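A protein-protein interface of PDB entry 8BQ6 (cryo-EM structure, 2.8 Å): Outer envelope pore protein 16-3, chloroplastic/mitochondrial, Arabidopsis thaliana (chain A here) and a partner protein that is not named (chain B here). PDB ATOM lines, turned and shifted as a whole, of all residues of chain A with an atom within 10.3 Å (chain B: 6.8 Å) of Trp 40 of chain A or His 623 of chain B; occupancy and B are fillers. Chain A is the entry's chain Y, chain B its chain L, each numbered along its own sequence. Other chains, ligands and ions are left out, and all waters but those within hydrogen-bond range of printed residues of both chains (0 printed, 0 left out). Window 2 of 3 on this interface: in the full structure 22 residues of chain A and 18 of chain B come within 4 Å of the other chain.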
ATOM      1  N   ILE A  32     -11.575 -29.868 -29.910  1.00  0.00           N
ATOM      2  CA  ILE A  32     -12.739 -30.179 -29.076  1.00  0.00           C
ATOM      3  C   ILE A  32     -12.838 -29.197 -27.910  1.00  0.00           C
ATOM      4  O   ILE A  32     -13.915 -28.654 -27.615  1.00  0.00           O
ATOM      5  CB  ILE A  32     -12.674 -31.641 -28.589  1.00  0.00           C
ATOM      6  CG1 ILE A  32     -13.338 -32.594 -29.589  1.00  0.00           C
ATOM      7  CG2 ILE A  32     -13.362 -31.801 -27.249  1.00  0.00           C
ATOM      8  CD1 ILE A  32     -12.906 -32.431 -31.020  1.00  0.00           C
ATOM      9  N   TYR A  33     -11.709 -28.938 -27.246  1.00  0.00           N
ATOM     10  CA  TYR A  33     -11.681 -28.031 -26.104  1.00  0.00           C
ATOM     11  C   TYR A  33     -12.069 -26.614 -26.515  1.00  0.00           C
ATOM     12  O   TYR A  33     -12.814 -25.931 -25.800  1.00  0.00           O
ATOM     13  CB  TYR A  33     -10.280 -28.050 -25.501  1.00  0.00           C
ATOM     14  CG  TYR A  33     -10.036 -27.133 -24.330  1.00  0.00           C
ATOM     15  CD1 TYR A  33      -8.861 -26.414 -24.243  1.00  0.00           C
ATOM     16  CD2 TYR A  33     -10.929 -27.053 -23.272  1.00  0.00           C
ATOM     17  CE1 TYR A  33      -8.596 -25.597 -23.172  1.00  0.00           C
ATOM     18  CE2 TYR A  33     -10.665 -26.241 -22.185  1.00  0.00           C
ATOM     19  CZ  TYR A  33      -9.499 -25.509 -22.146  1.00  0.00           C
ATOM     20  OH  TYR A  33      -9.214 -24.687 -21.079  1.00  0.00           O
ATOM     21  N   GLY A  34     -11.564 -26.155 -27.663  1.00  0.00           N
ATOM     22  CA  GLY A  34     -11.922 -24.836 -28.146  1.00  0.00           C
ATOM     23  C   GLY A  34     -13.393 -24.717 -28.487  1.00  0.00           C
ATOM     24  O   GLY A  34     -14.012 -23.682 -28.226  1.00  0.00           O
ATOM     25  N   THR A  35     -13.975 -25.770 -29.072  1.00  0.00           N
ATOM     26  CA  THR A  35     -15.414 -25.763 -29.328  1.00  0.00           C
ATOM     27  C   THR A  35     -16.199 -25.651 -28.028  1.00  0.00           C
ATOM     28  O   THR A  35     -17.159 -24.876 -27.929  1.00  0.00           O
ATOM     29  CB  THR A  35     -15.839 -27.028 -30.074  1.00  0.00           C
ATOM     30  OG1 THR A  35     -15.083 -27.169 -31.279  1.00  0.00           O
ATOM     31  CG2 THR A  35     -17.311 -26.952 -30.423  1.00  0.00           C
ATOM     32  N   ILE A  36     -15.809 -26.433 -27.020  1.00  0.00           N
ATOM     33  CA  ILE A  36     -16.528 -26.406 -25.749  1.00  0.00           C
ATOM     34  C   ILE A  36     -16.451 -25.018 -25.128  1.00  0.00           C
ATOM     35  O   ILE A  36     -17.460 -24.458 -24.679  1.00  0.00           O
ATOM     36  CB  ILE A  36     -15.985 -27.488 -24.800  1.00  0.00           C
ATOM     37  CG1 ILE A  36     -16.567 -28.850 -25.176  1.00  0.00           C
ATOM     38  CG2 ILE A  36     -16.296 -27.143 -23.356  1.00  0.00           C
ATOM     39  CD1 ILE A  36     -15.673 -30.011 -24.850  1.00  0.00           C
ATOM     40  N   LEU A  37     -15.255 -24.433 -25.117  1.00  0.00           N
ATOM     41  CA  LEU A  37     -15.080 -23.112 -24.523  1.00  0.00           C
ATOM     42  C   LEU A  37     -15.851 -22.048 -25.290  1.00  0.00           C
ATOM     43  O   LEU A  37     -16.415 -21.125 -24.695  1.00  0.00           O
ATOM     44  CB  LEU A  37     -13.599 -22.773 -24.467  1.00  0.00           C
ATOM     45  CG  LEU A  37     -13.089 -22.727 -23.041  1.00  0.00           C
ATOM     46  CD1 LEU A  37     -13.141 -24.107 -22.460  1.00  0.00           C
ATOM     47  CD2 LEU A  37     -11.674 -22.244 -23.089  1.00  0.00           C
ATOM     48  N   ALA A  38     -15.870 -22.147 -26.618  1.00  0.00           N
ATOM     49  CA  ALA A  38     -16.623 -21.179 -27.402  1.00  0.00           C
ATOM     50  C   ALA A  38     -18.118 -21.293 -27.126  1.00  0.00           C
ATOM     51  O   ALA A  38     -18.823 -20.279 -27.061  1.00  0.00           O
ATOM     52  CB  ALA A  38     -16.324 -21.366 -28.887  1.00  0.00           C
ATOM     53  N   THR A  39     -18.618 -22.521 -26.956  1.00  0.00           N
ATOM     54  CA  THR A  39     -20.045 -22.708 -26.710  1.00  0.00           C
ATOM     55  C   THR A  39     -20.449 -22.263 -25.307  1.00  0.00           C
ATOM     56  O   THR A  39     -21.550 -21.735 -25.124  1.00  0.00           O
ATOM     57  CB  THR A  39     -20.429 -24.170 -26.938  1.00  0.00           C
ATOM     58  OG1 THR A  39     -19.850 -24.627 -28.166  1.00  0.00           O
ATOM     59  CG2 THR A  39     -21.936 -24.316 -27.029  1.00  0.00           C
ATOM     60  N   TRP A  40     -19.577 -22.459 -24.312  1.00  0.00           N
ATOM     61  CA  TRP A  40     -19.895 -22.026 -22.952  1.00  0.00           C
ATOM     62  C   TRP A  40     -20.148 -20.521 -22.889  1.00  0.00           C
ATOM     63  O   TRP A  40     -21.111 -20.074 -22.254  1.00  0.00           O
ATOM     64  CB  TRP A  40     -18.763 -22.433 -22.005  1.00  0.00           C
ATOM     65  CG  TRP A  40     -19.116 -22.422 -20.542  1.00  0.00           C
ATOM     66  CD1 TRP A  40     -18.994 -21.371 -19.683  1.00  0.00           C
ATOM     67  CD2 TRP A  40     -19.630 -23.512 -19.767  1.00  0.00           C
ATOM     68  NE1 TRP A  40     -19.397 -21.736 -18.424  1.00  0.00           N
ATOM     69  CE2 TRP A  40     -19.799 -23.044 -18.450  1.00  0.00           C
ATOM     70  CE3 TRP A  40     -19.969 -24.835 -20.060  1.00  0.00           C
ATOM     71  CZ2 TRP A  40     -20.288 -23.850 -17.430  1.00  0.00           C
ATOM     72  CZ3 TRP A  40     -20.455 -25.632 -19.045  1.00  0.00           C
ATOM     73  CH2 TRP A  40     -20.610 -25.137 -17.745  1.00  0.00           C
ATOM     74  N   LYS A  41     -19.318 -19.729 -23.567  1.00  0.00           N
ATOM     75  CA  LYS A  41     -19.399 -18.272 -23.534  1.00  0.00           C
ATOM     76  C   LYS A  41     -20.702 -17.758 -24.145  1.00  0.00           C
ATOM     77  O   LYS A  41     -21.262 -18.341 -25.077  1.00  0.00           O
ATOM     78  CB  LYS A  41     -18.241 -17.650 -24.312  1.00  0.00           C
ATOM     79  CG  LYS A  41     -16.851 -18.029 -23.851  1.00  0.00           C
ATOM     80  CD  LYS A  41     -16.250 -16.976 -22.941  1.00  0.00           C
ATOM     81  CE  LYS A  41     -15.216 -17.587 -22.016  1.00  0.00           C
ATOM     82  NZ  LYS A  41     -13.817 -17.313 -22.435  1.00  0.00           N
ATOM     83  N   ASP A  42     -21.164 -16.626 -23.623  1.00  0.00           N
ATOM     84  CA  ASP A  42     -22.215 -15.849 -24.259  1.00  0.00           C
ATOM     85  C   ASP A  42     -21.641 -15.065 -25.437  1.00  0.00           C
ATOM     86  O   ASP A  42     -20.431 -15.038 -25.668  1.00  0.00           O
ATOM     87  CB  ASP A  42     -22.859 -14.896 -23.256  1.00  0.00           C
ATOM     88  CG  ASP A  42     -21.989 -13.686 -22.965  1.00  0.00           C
ATOM     89  OD1 ASP A  42     -20.911 -13.863 -22.358  1.00  0.00           O
ATOM     90  OD2 ASP A  42     -22.379 -12.559 -23.338  1.00  0.00           O
ATOM     91  N   VAL A  43     -22.527 -14.417 -26.188  1.00  0.00           N
ATOM     92  CA  VAL A  43     -22.093 -13.592 -27.314  1.00  0.00           C
ATOM     93  C   VAL A  43     -22.079 -12.127 -26.895  1.00  0.00           C
ATOM     94  O   VAL A  43     -22.935 -11.693 -26.109  1.00  0.00           O
ATOM     95  CB  VAL A  43     -22.975 -13.803 -28.555  1.00  0.00           C
ATOM     96  CG1 VAL A  43     -22.955 -15.258 -28.981  1.00  0.00           C
ATOM     97  CG2 VAL A  43     -24.401 -13.333 -28.302  1.00  0.00           C
ATOM     98  N   PRO A  44     -21.126 -11.338 -27.392  1.00  0.00           N
ATOM     99  CA  PRO A  44     -21.110  -9.906 -27.075  1.00  0.00           C
ATOM    100  C   PRO A  44     -22.403  -9.242 -27.518  1.00  0.00           C
ATOM    101  O   PRO A  44     -23.053  -9.672 -28.473  1.00  0.00           O
ATOM    102  CB  PRO A  44     -19.906  -9.373 -27.863  1.00  0.00           C
ATOM    103  CG  PRO A  44     -19.431 -10.505 -28.722  1.00  0.00           C
ATOM    104  CD  PRO A  44     -19.930 -11.768 -28.127  1.00  0.00           C
ATOM    105  N   ARG A  57     -15.791 -16.441 -34.577  1.00  0.00           N
ATOM    106  CA  ARG A  57     -15.086 -16.483 -33.301  1.00  0.00           C
ATOM    107  C   ARG A  57     -14.984 -17.911 -32.778  1.00  0.00           C
ATOM    108  O   ARG A  57     -13.951 -18.300 -32.219  1.00  0.00           O
ATOM    109  CB  ARG A  57     -15.783 -15.573 -32.293  1.00  0.00           C
ATOM    110  CG  ARG A  57     -15.802 -16.089 -30.869  1.00  0.00           C
ATOM    111  CD  ARG A  57     -16.844 -15.355 -30.038  1.00  0.00           C
ATOM    112  NE  ARG A  57     -16.499 -13.953 -29.838  1.00  0.00           N
ATOM    113  CZ  ARG A  57     -16.982 -12.947 -30.554  1.00  0.00           C
ATOM    114  NH1 ARG A  57     -17.869 -13.144 -31.515  1.00  0.00           N
ATOM    115  NH2 ARG A  57     -16.562 -11.710 -30.300  1.00  0.00           N
ATOM    116  N   THR A  58     -16.037 -18.711 -32.963  1.00  0.00           N
ATOM    117  CA  THR A  58     -15.979 -20.107 -32.537  1.00  0.00           C
ATOM    118  C   THR A  58     -14.892 -20.865 -33.293  1.00  0.00           C
ATOM    119  O   THR A  58     -14.106 -21.611 -32.695  1.00  0.00           O
ATOM    120  CB  THR A  58     -17.335 -20.778 -32.751  1.00  0.00           C
ATOM    121  OG1 THR A  58     -18.327 -20.124 -31.952  1.00  0.00           O
ATOM    122  CG2 THR A  58     -17.263 -22.234 -32.337  1.00  0.00           C
ATOM    123  N   MET A  61     -11.421 -19.766 -32.174  1.00  0.00           N
ATOM    124  CA  MET A  61     -11.073 -20.381 -30.899  1.00  0.00           C
ATOM    125  C   MET A  61     -10.702 -21.846 -31.096  1.00  0.00           C
ATOM    126  O   MET A  61      -9.734 -22.340 -30.501  1.00  0.00           O
ATOM    127  CB  MET A  61     -12.239 -20.224 -29.928  1.00  0.00           C
ATOM    128  CG  MET A  61     -11.988 -20.763 -28.547  1.00  0.00           C
ATOM    129  SD  MET A  61     -12.643 -19.631 -27.312  1.00  0.00           S
ATOM    130  CE  MET A  61     -11.647 -20.062 -25.896  1.00  0.00           C
ATOM    131  N   GLN B 615     -16.979 -20.066 -10.293  1.00  0.00           N
ATOM    132  CA  GLN B 615     -17.543 -19.412 -11.468  1.00  0.00           C
ATOM    133  C   GLN B 615     -18.194 -20.406 -12.422  1.00  0.00           C
ATOM    134  O   GLN B 615     -18.997 -20.011 -13.274  1.00  0.00           O
ATOM    135  CB  GLN B 615     -16.461 -18.614 -12.189  1.00  0.00           C
ATOM    136  CG  GLN B 615     -16.411 -17.156 -11.794  1.00  0.00           C
ATOM    137  CD  GLN B 615     -15.009 -16.596 -11.811  1.00  0.00           C
ATOM    138  OE1 GLN B 615     -14.197 -16.941 -12.668  1.00  0.00           O
ATOM    139  NE2 GLN B 615     -14.717 -15.715 -10.865  1.00  0.00           N
ATOM    140  N   LEU B 616     -17.855 -21.691 -12.301  1.00  0.00           N
ATOM    141  CA  LEU B 616     -18.481 -22.717 -13.130  1.00  0.00           C
ATOM    142  C   LEU B 616     -19.975 -22.812 -12.857  1.00  0.00           C
ATOM    143  O   LEU B 616     -20.776 -22.995 -13.783  1.00  0.00           O
ATOM    144  CB  LEU B 616     -17.816 -24.063 -12.869  1.00  0.00           C
ATOM    145  CG  LEU B 616     -16.793 -24.563 -13.877  1.00  0.00           C
ATOM    146  CD1 LEU B 616     -15.737 -23.505 -14.123  1.00  0.00           C
ATOM    147  CD2 LEU B 616     -16.166 -25.821 -13.325  1.00  0.00           C
ATOM    148  N   GLN B 617     -20.366 -22.713 -11.588  1.00  0.00           N
ATOM    149  CA  GLN B 617     -21.768 -22.657 -11.194  1.00  0.00           C
ATOM    150  C   GLN B 617     -22.345 -21.300 -11.564  1.00  0.00           C
ATOM    151  O   GLN B 617     -22.592 -20.461 -10.693  1.00  0.00           O
ATOM    152  CB  GLN B 617     -21.909 -22.906  -9.691  1.00  0.00           C
ATOM    153  CG  GLN B 617     -23.316 -23.238  -9.224  1.00  0.00           C
ATOM    154  CD  GLN B 617     -23.693 -24.674  -9.483  1.00  0.00           C
ATOM    155  OE1 GLN B 617     -22.846 -25.498  -9.819  1.00  0.00           O
ATOM    156  NE2 GLN B 617     -24.971 -24.988  -9.322  1.00  0.00           N
ATOM    157  N   SER B 618     -22.570 -21.083 -12.859  1.00  0.00           N
ATOM    158  CA  SER B 618     -22.848 -19.749 -13.372  1.00  0.00           C
ATOM    159  C   SER B 618     -24.258 -19.260 -13.070  1.00  0.00           C
ATOM    160  O   SER B 618     -24.528 -18.066 -13.232  1.00  0.00           O
ATOM    161  CB  SER B 618     -22.610 -19.719 -14.882  1.00  0.00           C
ATOM    162  OG  SER B 618     -23.504 -20.585 -15.555  1.00  0.00           O
ATOM    163  N   GLY B 619     -25.154 -20.138 -12.632  1.00  0.00           N
ATOM    164  CA  GLY B 619     -26.537 -19.768 -12.443  1.00  0.00           C
ATOM    165  C   GLY B 619     -27.405 -19.921 -13.669  1.00  0.00           C
ATOM    166  O   GLY B 619     -28.605 -19.627 -13.598  1.00  0.00           O
ATOM    167  N   PHE B 620     -26.849 -20.378 -14.782  1.00  0.00           N
ATOM    168  CA  PHE B 620     -27.605 -20.583 -16.007  1.00  0.00           C
ATOM    169  C   PHE B 620     -27.947 -22.061 -16.126  1.00  0.00           C
ATOM    170  O   PHE B 620     -27.058 -22.916 -16.055  1.00  0.00           O
ATOM    171  CB  PHE B 620     -26.811 -20.101 -17.216  1.00  0.00           C
ATOM    172  CG  PHE B 620     -26.703 -18.613 -17.297  1.00  0.00           C
ATOM    173  CD1 PHE B 620     -27.742 -17.856 -17.805  1.00  0.00           C
ATOM    174  CD2 PHE B 620     -25.579 -17.968 -16.827  1.00  0.00           C
ATOM    175  CE1 PHE B 620     -27.649 -16.485 -17.865  1.00  0.00           C
ATOM    176  CE2 PHE B 620     -25.481 -16.599 -16.884  1.00  0.00           C
ATOM    177  CZ  PHE B 620     -26.518 -15.855 -17.404  1.00  0.00           C
ATOM    178  N   VAL B 621     -29.238 -22.355 -16.287  1.00  0.00           N
ATOM    179  CA  VAL B 621     -29.685 -23.737 -16.414  1.00  0.00           C
ATOM    180  C   VAL B 621     -29.118 -24.380 -17.671  1.00  0.00           C
ATOM    181  O   VAL B 621     -28.926 -25.600 -17.721  1.00  0.00           O
ATOM    182  CB  VAL B 621     -31.224 -23.798 -16.395  1.00  0.00           C
ATOM    183  CG1 VAL B 621     -31.795 -23.160 -17.647  1.00  0.00           C
ATOM    184  CG2 VAL B 621     -31.701 -25.231 -16.260  1.00  0.00           C
ATOM    185  N   TYR B 622     -28.854 -23.581 -18.707  1.00  0.00           N
ATOM    186  CA  TYR B 622     -28.317 -24.137 -19.941  1.00  0.00           C
ATOM    187  C   TYR B 622     -26.929 -24.720 -19.718  1.00  0.00           C
ATOM    188  O   TYR B 622     -26.568 -25.736 -20.322  1.00  0.00           O
ATOM    189  CB  TYR B 622     -28.289 -23.066 -21.026  1.00  0.00           C
ATOM    190  CG  TYR B 622     -27.575 -23.487 -22.285  1.00  0.00           C
ATOM    191  CD1 TYR B 622     -28.198 -24.304 -23.218  1.00  0.00           C
ATOM    192  CD2 TYR B 622     -26.282 -23.064 -22.545  1.00  0.00           C
ATOM    193  CE1 TYR B 622     -27.553 -24.681 -24.374  1.00  0.00           C
ATOM    194  CE2 TYR B 622     -25.629 -23.445 -23.695  1.00  0.00           C
ATOM    195  CZ  TYR B 622     -26.269 -24.252 -24.605  1.00  0.00           C
ATOM    196  OH  TYR B 622     -25.618 -24.629 -25.753  1.00  0.00           O
ATOM    197  N   HIS B 623     -26.138 -24.093 -18.847  1.00  0.00           N
ATOM    198  CA  HIS B 623     -24.806 -24.610 -18.557  1.00  0.00           C
ATOM    199  C   HIS B 623     -24.877 -25.936 -17.817  1.00  0.00           C
ATOM    200  O   HIS B 623     -24.024 -26.805 -18.008  1.00  0.00           O
ATOM    201  CB  HIS B 623     -24.011 -23.587 -17.751  1.00  0.00           C
ATOM    202  CG  HIS B 623     -23.417 -22.497 -18.584  1.00  0.00           C
ATOM    203  ND1 HIS B 623     -23.325 -21.195 -18.147  1.00  0.00           N
ATOM    204  CD2 HIS B 623     -22.876 -22.517 -19.825  1.00  0.00           C
ATOM    205  CE1 HIS B 623     -22.756 -20.457 -19.083  1.00  0.00           C
ATOM    206  NE2 HIS B 623     -22.474 -21.236 -20.112  1.00  0.00           N
ATOM    207  N   TYR B 624     -25.896 -26.117 -16.979  1.00  0.00           N
ATOM    208  CA  TYR B 624     -26.018 -27.363 -16.228  1.00  0.00           C
ATOM    209  C   TYR B 624     -26.388 -28.516 -17.151  1.00  0.00           C
ATOM    210  O   TYR B 624     -25.834 -29.620 -17.042  1.00  0.00           O
ATOM    211  CB  TYR B 624     -27.057 -27.195 -15.121  1.00  0.00           C
ATOM    212  CG  TYR B 624     -26.758 -26.064 -14.158  1.00  0.00           C
ATOM    213  CD1 TYR B 624     -25.539 -25.395 -14.189  1.00  0.00           C
ATOM    214  CD2 TYR B 624     -27.710 -25.637 -13.248  1.00  0.00           C
ATOM    215  CE1 TYR B 624     -25.271 -24.360 -13.330  1.00  0.00           C
ATOM    216  CE2 TYR B 624     -27.449 -24.599 -12.382  1.00  0.00           C
ATOM    217  CZ  TYR B 624     -26.228 -23.965 -12.430  1.00  0.00           C
ATOM    218  OH  TYR B 624     -25.961 -22.929 -11.569  1.00  0.00           O
ATOM    219  N   ALA B 625     -27.309 -28.268 -18.084  1.00  0.00           N
ATOM    220  CA  ALA B 625     -27.645 -29.265 -19.092  1.00  0.00           C
ATOM    221  C   ALA B 625     -26.461 -29.544 -20.007  1.00  0.00           C
ATOM    222  O   ALA B 625     -26.207 -30.698 -20.369  1.00  0.00           O
ATOM    223  CB  ALA B 625     -28.851 -28.800 -19.902  1.00  0.00           C
ATOM    224  N   PHE B 626     -25.733 -28.497 -20.398  1.00  0.00           N
ATOM    225  CA  PHE B 626     -24.550 -28.684 -21.227  1.00  0.00           C
ATOM    226  C   PHE B 626     -23.502 -29.520 -20.504  1.00  0.00           C
ATOM    227  O   PHE B 626     -22.863 -30.383 -21.110  1.00  0.00           O
ATOM    228  CB  PHE B 626     -23.976 -27.325 -21.626  1.00  0.00           C
ATOM    229  CG  PHE B 626     -22.963 -27.392 -22.731  1.00  0.00           C
ATOM    230  CD1 PHE B 626     -22.971 -28.430 -23.646  1.00  0.00           C
ATOM    231  CD2 PHE B 626     -21.962 -26.443 -22.816  1.00  0.00           C
ATOM    232  CE1 PHE B 626     -22.022 -28.491 -24.652  1.00  0.00           C
ATOM    233  CE2 PHE B 626     -21.013 -26.502 -23.814  1.00  0.00           C
ATOM    234  CZ  PHE B 626     -21.041 -27.526 -24.730  1.00  0.00           C
ATOM    235  N   ALA B 627     -23.316 -29.281 -19.204  1.00  0.00           N
ATOM    236  CA  ALA B 627     -22.385 -30.085 -18.420  1.00  0.00           C
ATOM    237  C   ALA B 627     -22.832 -31.538 -18.346  1.00  0.00           C
ATOM    238  O   ALA B 627     -22.009 -32.453 -18.466  1.00  0.00           O
ATOM    239  CB  ALA B 627     -22.241 -29.501 -17.018  1.00  0.00           C
ATOM    240  N   MET B 628     -24.129 -31.773 -18.136  1.00  0.00           N
ATOM    241  CA  MET B 628     -24.624 -33.149 -18.129  1.00  0.00           C
ATOM    242  C   MET B 628     -24.377 -33.828 -19.471  1.00  0.00           C
ATOM    243  O   MET B 628     -23.937 -34.984 -19.526  1.00  0.00           O
ATOM    244  CB  MET B 628     -26.112 -33.169 -17.788  1.00  0.00           C
ATOM    245  CG  MET B 628     -26.415 -32.866 -16.339  1.00  0.00           C
ATOM    246  SD  MET B 628     -28.177 -32.649 -16.025  1.00  0.00           S
ATOM    247  CE  MET B 628     -28.833 -34.203 -16.622  1.00  0.00           C
ATOM    248  N   LEU B 630     -22.101 -33.059 -21.721  1.00  0.00           N
ATOM    249  CA  LEU B 630     -20.669 -33.264 -21.891  1.00  0.00           C
ATOM    250  C   LEU B 630     -20.186 -34.458 -21.085  1.00  0.00           C
ATOM    251  O   LEU B 630     -19.334 -35.219 -21.547  1.00  0.00           O
ATOM    252  CB  LEU B 630     -19.910 -32.007 -21.479  1.00  0.00           C
ATOM    253  CG  LEU B 630     -19.961 -30.840 -22.457  1.00  0.00           C
ATOM    254  CD1 LEU B 630     -19.216 -29.666 -21.861  1.00  0.00           C
ATOM    255  CD2 LEU B 630     -19.373 -31.234 -23.800  1.00  0.00           C
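Among the printed residues, pairs that only touch across the chains: Ile 36 of chain A with Leu 630 of chain B (3.9 Å), Thr 39 of chain A with Tyr 622 of chain B (3.9 Å), Thr 39 of chain A with Phe 626 of chain B (3.9 Å), Trp 40 of chain A with Leu 616 of chain B (3.8 Å) and Trp 40 of chain A with Phe 626 of chain B (3.8 Å).
Hydrophobic or aromatic side chains of chain B that line the printed part of chain A: Tyr 622, His 623, Phe 626 and Leu 630. Along chain B the printed residues that touch a printed residue of chain A span positions 616 to 630. Of the 16 printed residues of chain A, 3 touch a printed residue of chain B. Hydrophobic or aromatic side chains of chain A within 4 Å of the printed part of chain B: Ile 36 and Trp 40.
The backbone carbonyl oxygen (O) of Thr 35 of chain A is in hydrogen-bond range of the side-chain hydroxyl (OG1) of Thr 39 of chain A, at 2.7 Å. The side-chain hydroxyl (OG) of Ser 618 of chain B is in hydrogen-bond range of a ring nitrogen (ND1) of His 623 of chain B, at 2.7 Å.
Of chain B, only Leu 616 (3.8 Å), His 623 (2.8 Å) and Phe 626 (3.8 Å) come within 4 Å of Trp 40 of chain A. Leu 616 of chain B touches one residue of chain A. No residue of chain A comes within 4 Å of Val 621 of chain B. No residue of chain A comes within 4 Å of Ala 625 of chain B. Phe 626 of chain B touches just these residues of chain A: Thr 39 and Trp 40. Of the printed residues of chain A, Leu 630 of chain B touches Ile 36. Of the printed residues of chain B, Ile 36 of chain A touches Leu 630. Of the printed residues of chain A, Tyr 622 of chain B touches Thr 39 (3.9 Å). Tyr 624 of chain B touches none of the printed residues of chain A. Phe 620 of chain B touches none of the printed residues of chain A. The nearest residue of chain B that does not touch Trp 40 of chain A is Ala 627 of chain B (4.6 Å). The nearest printed residue of chain B that does not touch Ile 36 of chain A is Phe 626 of chain B (4.2 Å).
NE2 of His 623 of chain B sits at hydrogen-bond distance from O of Trp 40 of chain A (2.8 Å).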
